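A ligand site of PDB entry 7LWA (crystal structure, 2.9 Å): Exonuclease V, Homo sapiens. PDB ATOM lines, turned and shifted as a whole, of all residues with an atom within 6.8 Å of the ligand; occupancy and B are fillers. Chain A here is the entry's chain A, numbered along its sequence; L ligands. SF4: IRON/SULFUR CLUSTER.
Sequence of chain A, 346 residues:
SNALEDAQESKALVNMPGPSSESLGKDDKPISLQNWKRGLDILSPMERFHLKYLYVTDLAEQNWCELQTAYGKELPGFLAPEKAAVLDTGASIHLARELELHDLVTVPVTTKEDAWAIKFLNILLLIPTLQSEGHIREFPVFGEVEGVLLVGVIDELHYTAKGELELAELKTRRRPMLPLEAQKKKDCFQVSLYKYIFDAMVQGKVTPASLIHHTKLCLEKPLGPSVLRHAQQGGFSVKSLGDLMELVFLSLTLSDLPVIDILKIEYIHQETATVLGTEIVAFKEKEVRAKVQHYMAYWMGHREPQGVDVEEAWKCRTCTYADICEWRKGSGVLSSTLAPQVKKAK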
ATOM      1  N   TRP A  64      38.772  17.148  -5.518  1.00  0.00           N
ATOM      2  CA  TRP A  64      37.581  16.592  -6.135  1.00  0.00           C
ATOM      3  C   TRP A  64      36.756  17.693  -6.809  1.00  0.00           C
ATOM      4  O   TRP A  64      36.498  17.647  -8.013  1.00  0.00           O
ATOM      5  CB  TRP A  64      36.750  15.854  -5.091  1.00  0.00           C
ATOM      6  CG  TRP A  64      35.507  15.217  -5.633  1.00  0.00           C
ATOM      7  CD1 TRP A  64      34.250  15.763  -5.658  1.00  0.00           C
ATOM      8  CD2 TRP A  64      35.383  13.915  -6.208  1.00  0.00           C
ATOM      9  NE1 TRP A  64      33.369  14.879  -6.220  1.00  0.00           N
ATOM     10  CE2 TRP A  64      34.036  13.734  -6.575  1.00  0.00           C
ATOM     11  CE3 TRP A  64      36.298  12.886  -6.459  1.00  0.00           C
ATOM     12  CZ2 TRP A  64      33.569  12.571  -7.176  1.00  0.00           C
ATOM     13  CZ3 TRP A  64      35.830  11.724  -7.060  1.00  0.00           C
ATOM     14  CH2 TRP A  64      34.484  11.580  -7.409  1.00  0.00           C
ATOM     15  N   CYS A  65      36.344  18.691  -6.031  1.00  0.00           N
ATOM     16  CA  CYS A  65      35.723  19.884  -6.579  1.00  0.00           C
ATOM     17  C   CYS A  65      35.972  21.041  -5.627  1.00  0.00           C
ATOM     18  O   CYS A  65      35.624  20.959  -4.444  1.00  0.00           O
ATOM     19  CB  CYS A  65      34.215  19.693  -6.782  1.00  0.00           C
ATOM     20  SG  CYS A  65      33.425  21.162  -7.476  1.00  0.00           S
ATOM     21  N   GLU A  66      36.590  22.108  -6.140  1.00  0.00           N
ATOM     22  CA  GLU A  66      36.848  23.281  -5.307  1.00  0.00           C
ATOM     23  C   GLU A  66      35.554  24.003  -4.951  1.00  0.00           C
ATOM     24  O   GLU A  66      35.395  24.484  -3.828  1.00  0.00           O
ATOM     25  CB  GLU A  66      37.819  24.214  -6.036  1.00  0.00           C
ATOM     26  CG  GLU A  66      38.100  25.524  -5.327  1.00  0.00           C
ATOM     27  CD  GLU A  66      39.265  26.261  -5.953  1.00  0.00           C
ATOM     28  OE1 GLU A  66      40.382  26.204  -5.387  1.00  0.00           O
ATOM     29  OE2 GLU A  66      39.074  26.890  -7.012  1.00  0.00           O
ATOM     30  N   LEU A  67      34.620  24.073  -5.894  1.00  0.00           N
ATOM     31  CA  LEU A  67      33.348  24.750  -5.633  1.00  0.00           C
ATOM     32  C   LEU A  67      32.499  23.971  -4.631  1.00  0.00           C
ATOM     33  O   LEU A  67      31.864  24.568  -3.758  1.00  0.00           O
ATOM     34  CB  LEU A  67      32.591  24.961  -6.944  1.00  0.00           C
ATOM     35  CG  LEU A  67      31.599  26.125  -6.993  1.00  0.00           C
ATOM     36  CD1 LEU A  67      32.139  27.321  -6.238  1.00  0.00           C
ATOM     37  CD2 LEU A  67      31.311  26.488  -8.436  1.00  0.00           C
ATOM     38  N   GLN A  68      32.474  22.644  -4.766  1.00  0.00           N
ATOM     39  CA  GLN A  68      31.730  21.818  -3.818  1.00  0.00           C
ATOM     40  C   GLN A  68      32.318  21.934  -2.414  1.00  0.00           C
ATOM     41  O   GLN A  68      31.585  21.933  -1.417  1.00  0.00           O
ATOM     42  CB  GLN A  68      31.718  20.372  -4.290  1.00  0.00           C
ATOM     43  CG  GLN A  68      31.261  19.351  -3.268  1.00  0.00           C
ATOM     44  CD  GLN A  68      31.485  17.928  -3.736  1.00  0.00           C
ATOM     45  OE1 GLN A  68      32.389  17.245  -3.257  1.00  0.00           O
ATOM     46  NE2 GLN A  68      30.669  17.477  -4.682  1.00  0.00           N
ATOM     47  N   THR A  69      33.645  22.030  -2.315  1.00  0.00           N
ATOM     48  CA  THR A  69      34.279  22.238  -1.018  1.00  0.00           C
ATOM     49  C   THR A  69      33.935  23.603  -0.444  1.00  0.00           C
ATOM     50  O   THR A  69      33.720  23.747   0.769  1.00  0.00           O
ATOM     51  CB  THR A  69      35.790  22.065  -1.144  1.00  0.00           C
ATOM     52  OG1 THR A  69      36.087  20.751  -1.619  1.00  0.00           O
ATOM     53  CG2 THR A  69      36.476  22.274   0.190  1.00  0.00           C
ATOM     54  N   TYR A  71      31.145  25.374  -1.033  1.00  0.00           N
ATOM     55  CA  TYR A  71      29.770  25.272  -0.555  1.00  0.00           C
ATOM     56  C   TYR A  71      29.693  24.482   0.744  1.00  0.00           C
ATOM     57  O   TYR A  71      28.850  24.787   1.598  1.00  0.00           O
ATOM     58  CB  TYR A  71      28.892  24.613  -1.623  1.00  0.00           C
ATOM     59  CG  TYR A  71      28.538  25.514  -2.782  1.00  0.00           C
ATOM     60  CD1 TYR A  71      28.039  26.792  -2.578  1.00  0.00           C
ATOM     61  CD2 TYR A  71      28.695  25.078  -4.095  1.00  0.00           C
ATOM     62  CE1 TYR A  71      27.707  27.617  -3.643  1.00  0.00           C
ATOM     63  CE2 TYR A  71      28.369  25.896  -5.163  1.00  0.00           C
ATOM     64  CZ  TYR A  71      27.885  27.157  -4.930  1.00  0.00           C
ATOM     65  OH  TYR A  71      27.554  27.967  -5.993  1.00  0.00           O
ATOM     66  N   GLN A 306      36.711  27.316  -8.582  1.00  0.00           N
ATOM     67  CA  GLN A 306      36.410  26.640  -9.832  1.00  0.00           C
ATOM     68  C   GLN A 306      35.594  25.380  -9.580  1.00  0.00           C
ATOM     69  O   GLN A 306      35.756  24.702  -8.567  1.00  0.00           O
ATOM     70  CB  GLN A 306      37.693  26.262 -10.579  1.00  0.00           C
ATOM     71  CG  GLN A 306      38.809  27.289 -10.475  1.00  0.00           C
ATOM     72  CD  GLN A 306      38.594  28.474 -11.394  1.00  0.00           C
ATOM     73  OE1 GLN A 306      37.787  28.410 -12.333  1.00  0.00           O
ATOM     74  NE2 GLN A 306      39.296  29.559 -11.132  1.00  0.00           N
ATOM     75  N   GLY A 307      34.694  25.084 -10.516  1.00  0.00           N
ATOM     76  CA  GLY A 307      33.999  23.823 -10.534  1.00  0.00           C
ATOM     77  C   GLY A 307      34.822  22.754 -11.233  1.00  0.00           C
ATOM     78  O   GLY A 307      35.975  22.961 -11.621  1.00  0.00           O
ATOM     79  N   VAL A 308      34.201  21.592 -11.405  1.00  0.00           N
ATOM     80  CA  VAL A 308      34.885  20.480 -12.060  1.00  0.00           C
ATOM     81  C   VAL A 308      34.921  20.716 -13.564  1.00  0.00           C
ATOM     82  O   VAL A 308      34.118  21.462 -14.137  1.00  0.00           O
ATOM     83  CB  VAL A 308      34.226  19.132 -11.721  1.00  0.00           C
ATOM     84  CG1 VAL A 308      34.197  18.925 -10.227  1.00  0.00           C
ATOM     85  CG2 VAL A 308      32.821  19.073 -12.300  1.00  0.00           C
ATOM     86  N   GLU A 312      34.569  15.686 -16.313  1.00  0.00           N
ATOM     87  CA  GLU A 312      34.169  15.148 -15.011  1.00  0.00           C
ATOM     88  C   GLU A 312      32.835  15.729 -14.556  1.00  0.00           C
ATOM     89  O   GLU A 312      32.625  15.930 -13.354  1.00  0.00           O
ATOM     90  CB  GLU A 312      35.260  15.411 -13.971  1.00  0.00           C
ATOM     91  CG  GLU A 312      36.539  14.630 -14.221  1.00  0.00           C
ATOM     92  CD  GLU A 312      37.429  14.557 -13.000  1.00  0.00           C
ATOM     93  OE1 GLU A 312      37.428  15.516 -12.198  1.00  0.00           O
ATOM     94  OE2 GLU A 312      38.135  13.538 -12.822  1.00  0.00           O
ATOM     95  N   ALA A 313      31.937  16.018 -15.497  1.00  0.00           N
ATOM     96  CA  ALA A 313      30.630  16.567 -15.154  1.00  0.00           C
ATOM     97  C   ALA A 313      29.753  15.582 -14.409  1.00  0.00           C
ATOM     98  O   ALA A 313      28.746  15.977 -13.822  1.00  0.00           O
ATOM     99  CB  ALA A 313      29.914  17.051 -16.413  1.00  0.00           C
ATOM    100  N   LYS A 315      30.420  14.270 -11.705  1.00  0.00           N
ATOM    101  CA  LYS A 315      30.589  14.478 -10.265  1.00  0.00           C
ATOM    102  C   LYS A 315      29.398  15.221  -9.677  1.00  0.00           C
ATOM    103  O   LYS A 315      29.111  15.069  -8.478  1.00  0.00           O
ATOM    104  CB  LYS A 315      31.877  15.252  -9.998  1.00  0.00           C
ATOM    105  CG  LYS A 315      33.144  14.437 -10.185  1.00  0.00           C
ATOM    106  CD  LYS A 315      34.375  15.333 -10.130  1.00  0.00           C
ATOM    107  CE  LYS A 315      35.602  14.582  -9.683  1.00  0.00           C
ATOM    108  NZ  LYS A 315      36.787  15.476  -9.570  1.00  0.00           N
ATOM    109  N   CYS A 316      28.699  16.016 -10.478  1.00  0.00           N
ATOM    110  CA  CYS A 316      27.571  16.810 -10.004  1.00  0.00           C
ATOM    111  C   CYS A 316      26.275  16.013  -9.942  1.00  0.00           C
ATOM    112  O   CYS A 316      25.298  16.498  -9.353  1.00  0.00           O
ATOM    113  CB  CYS A 316      27.369  18.033 -10.913  1.00  0.00           C
ATOM    114  SG  CYS A 316      28.904  18.743 -11.562  1.00  0.00           S
ATOM    115  N   ARG A 317      26.238  14.814 -10.520  1.00  0.00           N
ATOM    116  CA  ARG A 317      25.053  13.976 -10.431  1.00  0.00           C
ATOM    117  C   ARG A 317      24.699  13.675  -8.976  1.00  0.00           C
ATOM    118  O   ARG A 317      23.513  13.539  -8.638  1.00  0.00           O
ATOM    119  CB  ARG A 317      25.259  12.674 -11.202  1.00  0.00           C
ATOM    120  CG  ARG A 317      25.101  12.792 -12.711  1.00  0.00           C
ATOM    121  CD  ARG A 317      25.764  11.616 -13.428  1.00  0.00           C
ATOM    122  NE  ARG A 317      25.458  10.339 -12.794  1.00  0.00           N
ATOM    123  CZ  ARG A 317      24.652   9.417 -13.317  1.00  0.00           C
ATOM    124  NH1 ARG A 317      24.434   8.281 -12.667  1.00  0.00           N
ATOM    125  NH2 ARG A 317      24.065   9.631 -14.489  1.00  0.00           N
ATOM    126  N   THR A 318      25.702  13.566  -8.113  1.00  0.00           N
ATOM    127  CA  THR A 318      25.506  13.253  -6.706  1.00  0.00           C
ATOM    128  C   THR A 318      25.919  14.401  -5.793  1.00  0.00           C
ATOM    129  O   THR A 318      25.926  14.224  -4.563  1.00  0.00           O
ATOM    130  CB  THR A 318      26.269  11.982  -6.332  1.00  0.00           C
ATOM    131  OG1 THR A 318      27.575  12.025  -6.914  1.00  0.00           O
ATOM    132  CG2 THR A 318      25.537  10.756  -6.835  1.00  0.00           C
ATOM    133  N   CYS A 319      26.270  15.553  -6.341  1.00  0.00           N
ATOM    134  CA  CYS A 319      26.705  16.662  -5.512  1.00  0.00           C
ATOM    135  C   CYS A 319      25.533  17.268  -4.755  1.00  0.00           C
ATOM    136  O   CYS A 319      24.449  17.480  -5.319  1.00  0.00           O
ATOM    137  CB  CYS A 319      27.377  17.742  -6.362  1.00  0.00           C
ATOM    138  SG  CYS A 319      27.896  19.204  -5.436  1.00  0.00           S
ATOM    139  N   THR A 320      25.745  17.543  -3.468  1.00  0.00           N
ATOM    140  CA  THR A 320      24.680  18.090  -2.629  1.00  0.00           C
ATOM    141  C   THR A 320      24.203  19.431  -3.154  1.00  0.00           C
ATOM    142  O   THR A 320      23.002  19.731  -3.106  1.00  0.00           O
ATOM    143  CB  THR A 320      25.171  18.239  -1.186  1.00  0.00           C
ATOM    144  OG1 THR A 320      25.827  17.035  -0.772  1.00  0.00           O
ATOM    145  CG2 THR A 320      24.011  18.530  -0.253  1.00  0.00           C
ATOM    146  N   TYR A 321      25.109  20.248  -3.684  1.00  0.00           N
ATOM    147  CA  TYR A 321      24.817  21.613  -4.083  1.00  0.00           C
ATOM    148  C   TYR A 321      24.607  21.768  -5.587  1.00  0.00           C
ATOM    149  O   TYR A 321      24.761  22.867  -6.124  1.00  0.00           O
ATOM    150  CB  TYR A 321      25.936  22.544  -3.609  1.00  0.00           C
ATOM    151  CG  TYR A 321      26.422  22.224  -2.213  1.00  0.00           C
ATOM    152  CD1 TYR A 321      25.795  22.767  -1.092  1.00  0.00           C
ATOM    153  CD2 TYR A 321      27.486  21.366  -2.005  1.00  0.00           C
ATOM    154  CE1 TYR A 321      26.225  22.475   0.180  1.00  0.00           C
ATOM    155  CE2 TYR A 321      27.930  21.055  -0.728  1.00  0.00           C
ATOM    156  CZ  TYR A 321      27.289  21.616   0.364  1.00  0.00           C
ATOM    157  OH  TYR A 321      27.725  21.317   1.631  1.00  0.00           O
ATOM    158  N   ALA A 322      24.258  20.680  -6.270  1.00  0.00           N
ATOM    159  CA  ALA A 322      24.041  20.751  -7.719  1.00  0.00           C
ATOM    160  C   ALA A 322      22.808  21.556  -8.084  1.00  0.00           C
ATOM    161  O   ALA A 322      22.677  21.979  -9.241  1.00  0.00           O
ATOM    162  CB  ALA A 322      23.938  19.336  -8.303  1.00  0.00           C
ATOM    163  N   ASP A 323      21.910  21.796  -7.131  1.00  0.00           N
ATOM    164  CA  ASP A 323      20.657  22.490  -7.416  1.00  0.00           C
ATOM    165  C   ASP A 323      20.774  24.003  -7.337  1.00  0.00           C
ATOM    166  O   ASP A 323      19.815  24.707  -7.707  1.00  0.00           O
ATOM    167  CB  ASP A 323      19.564  22.020  -6.450  1.00  0.00           C
ATOM    168  CG  ASP A 323      20.068  21.841  -5.027  1.00  0.00           C
ATOM    169  OD1 ASP A 323      21.294  21.723  -4.837  1.00  0.00           O
ATOM    170  OD2 ASP A 323      19.227  21.815  -4.098  1.00  0.00           O
ATOM    171  N   CYS A 325      24.211  25.373  -7.824  1.00  0.00           N
ATOM    172  CA  CYS A 325      25.542  25.628  -8.382  1.00  0.00           C
ATOM    173  C   CYS A 325      25.372  26.209  -9.782  1.00  0.00           C
ATOM    174  O   CYS A 325      24.919  25.513 -10.700  1.00  0.00           O
ATOM    175  CB  CYS A 325      26.390  24.362  -8.414  1.00  0.00           C
ATOM    176  SG  CYS A 325      27.991  24.541  -9.249  1.00  0.00           S
ATOM    177  N   GLU A 326      25.729  27.472  -9.945  1.00  0.00           N
ATOM    178  CA  GLU A 326      25.637  28.134 -11.240  1.00  0.00           C
ATOM    179  C   GLU A 326      26.808  27.802 -12.161  1.00  0.00           C
ATOM    180  O   GLU A 326      26.818  28.258 -13.311  1.00  0.00           O
ATOM    181  CB  GLU A 326      25.527  29.646 -11.051  1.00  0.00           C
ATOM    182  CG  GLU A 326      24.093  30.137 -10.917  1.00  0.00           C
ATOM    183  CD  GLU A 326      23.573  30.041  -9.501  1.00  0.00           C
ATOM    184  OE1 GLU A 326      24.113  30.731  -8.607  1.00  0.00           O
ATOM    185  OE2 GLU A 326      22.613  29.270  -9.260  1.00  0.00           O
ATOM    186  N   TRP A 327      27.793  27.037 -11.689  1.00  0.00           N
ATOM    187  CA  TRP A 327      28.834  26.534 -12.567  1.00  0.00           C
ATOM    188  C   TRP A 327      28.325  25.372 -13.409  1.00  0.00           C
ATOM    189  O   TRP A 327      28.612  25.295 -14.611  1.00  0.00           O
ATOM    190  CB  TRP A 327      30.053  26.099 -11.743  1.00  0.00           C
ATOM    191  CG  TRP A 327      31.181  25.513 -12.534  1.00  0.00           C
ATOM    192  CD1 TRP A 327      31.238  24.263 -13.096  1.00  0.00           C
ATOM    193  CD2 TRP A 327      32.445  26.134 -12.829  1.00  0.00           C
ATOM    194  NE1 TRP A 327      32.438  24.081 -13.740  1.00  0.00           N
ATOM    195  CE2 TRP A 327      33.198  25.209 -13.587  1.00  0.00           C
ATOM    196  CE3 TRP A 327      32.993  27.380 -12.532  1.00  0.00           C
ATOM    197  CZ2 TRP A 327      34.485  25.501 -14.045  1.00  0.00           C
ATOM    198  CZ3 TRP A 327      34.270  27.663 -12.994  1.00  0.00           C
ATOM    199  CH2 TRP A 327      35.001  26.722 -13.734  1.00  0.00           C
ATOM    200  N   ARG A 328      27.559  24.464 -12.792  1.00  0.00           N
ATOM    201  CA  ARG A 328      26.962  23.355 -13.531  1.00  0.00           C
ATOM    202  C   ARG A 328      25.954  23.859 -14.564  1.00  0.00           C
ATOM    203  O   ARG A 328      25.739  23.208 -15.594  1.00  0.00           O
ATOM    204  CB  ARG A 328      26.300  22.383 -12.558  1.00  0.00           C
ATOM    205  CG  ARG A 328      25.801  21.100 -13.192  1.00  0.00           C
ATOM    206  CD  ARG A 328      24.878  20.351 -12.241  1.00  0.00           C
ATOM    207  NE  ARG A 328      23.867  21.238 -11.666  1.00  0.00           N
ATOM    208  CZ  ARG A 328      22.756  21.613 -12.297  1.00  0.00           C
ATOM    209  NH1 ARG A 328      22.512  21.181 -13.526  1.00  0.00           N
ATOM    210  NH2 ARG A 328      21.895  22.421 -11.692  1.00  0.00           N
HETATM  211 FE1  SF4 L   1      28.794  20.341  -7.181  1.00  0.00          FE
HETATM  212 FE2  SF4 L   1      29.474  20.072  -9.814  1.00  0.00          FE
HETATM  213 FE3  SF4 L   1      31.233  21.209  -8.059  1.00  0.00          FE
HETATM  214 FE4  SF4 L   1      28.958  22.543  -8.796  1.00  0.00          FE
HETATM  215  S1  SF4 L   1      30.704  21.964 -10.146  1.00  0.00           S
HETATM  216  S2  SF4 L   1      29.797  22.322  -6.689  1.00  0.00           S
HETATM  217  S3  SF4 L   1      27.482  20.815  -8.981  1.00  0.00           S
HETATM  218  S4  SF4 L   1      30.481  19.066  -8.025  1.00  0.00           S
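The backbone NH (N) of Trp 327 lies close to the side-chain sulfur (SG) of Cys 325 (3.5 Å).
The side-chain sulfur of Cys 325 lies close to the backbone NH of Arg 328 (3.6 Å).
The backbone carbonyl oxygen (O) of Ala 313 lies close to the side-chain sulfur (SG) of Cys 316 (3.6 Å).
The side-chain sulfur of Cys 65 sits close to the backbone NH of Leu 67 (3.5 Å).
The side-chain hydroxyl (OG1) of Thr 69 is in hydrogen-bond range of the backbone carbonyl oxygen (O) of Cys 65, 2.9 Å away.
The backbone carbonyl oxygen (O) of Ala 322 sits at hydrogen-bond distance from the guanidinium group (NH2) of Arg 328 (2.6 Å).
NE1 of Trp 327 is in hydrogen-bond range of O of Val 308, at 3.1 Å.
The backbone NH (N) of Leu 67 sits at hydrogen-bond distance from the backbone carbonyl oxygen (O) of Gln 306, 3.0 Å away.
Merely in contact with the ligand: Leu 67, Tyr 71, Gly 307, Ala 322 and Trp 327.
Hydrophobic or aromatic side chains within 4 Å of the ligand: Leu 67, Tyr 71, Ala 322 and Trp 327.
11 residues have an atom within 4 Å of the ligand: Cys 65, Leu 67, Gln 68, Tyr 71, Gly 307, Val 308, Cys 316, Cys 319, Ala 322, Cys 325 and Trp 327.
SG of Cys 325 binds FE4 of the ligand, 2.3 Å away.
An iron atom (FE1) of the ligand is bound by the side-chain sulfur (SG) of Cys 319 (2.3 Å).
An iron atom (FE2) of the ligand is bound by the side-chain sulfur (SG) of Cys 316.
The side-chain sulfur (SG) of Cys 65 binds an iron atom (FE3) of the ligand.
A sulfur (S2) of the ligand sits close to the backbone NH (N) of Gln 68, 3.3 Å away.
NE2 of Gln 68 sits close to S4 of the ligand (3.7 Å).
N of Val 308 lies close to S1 of the ligand, at 3.7 Å.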
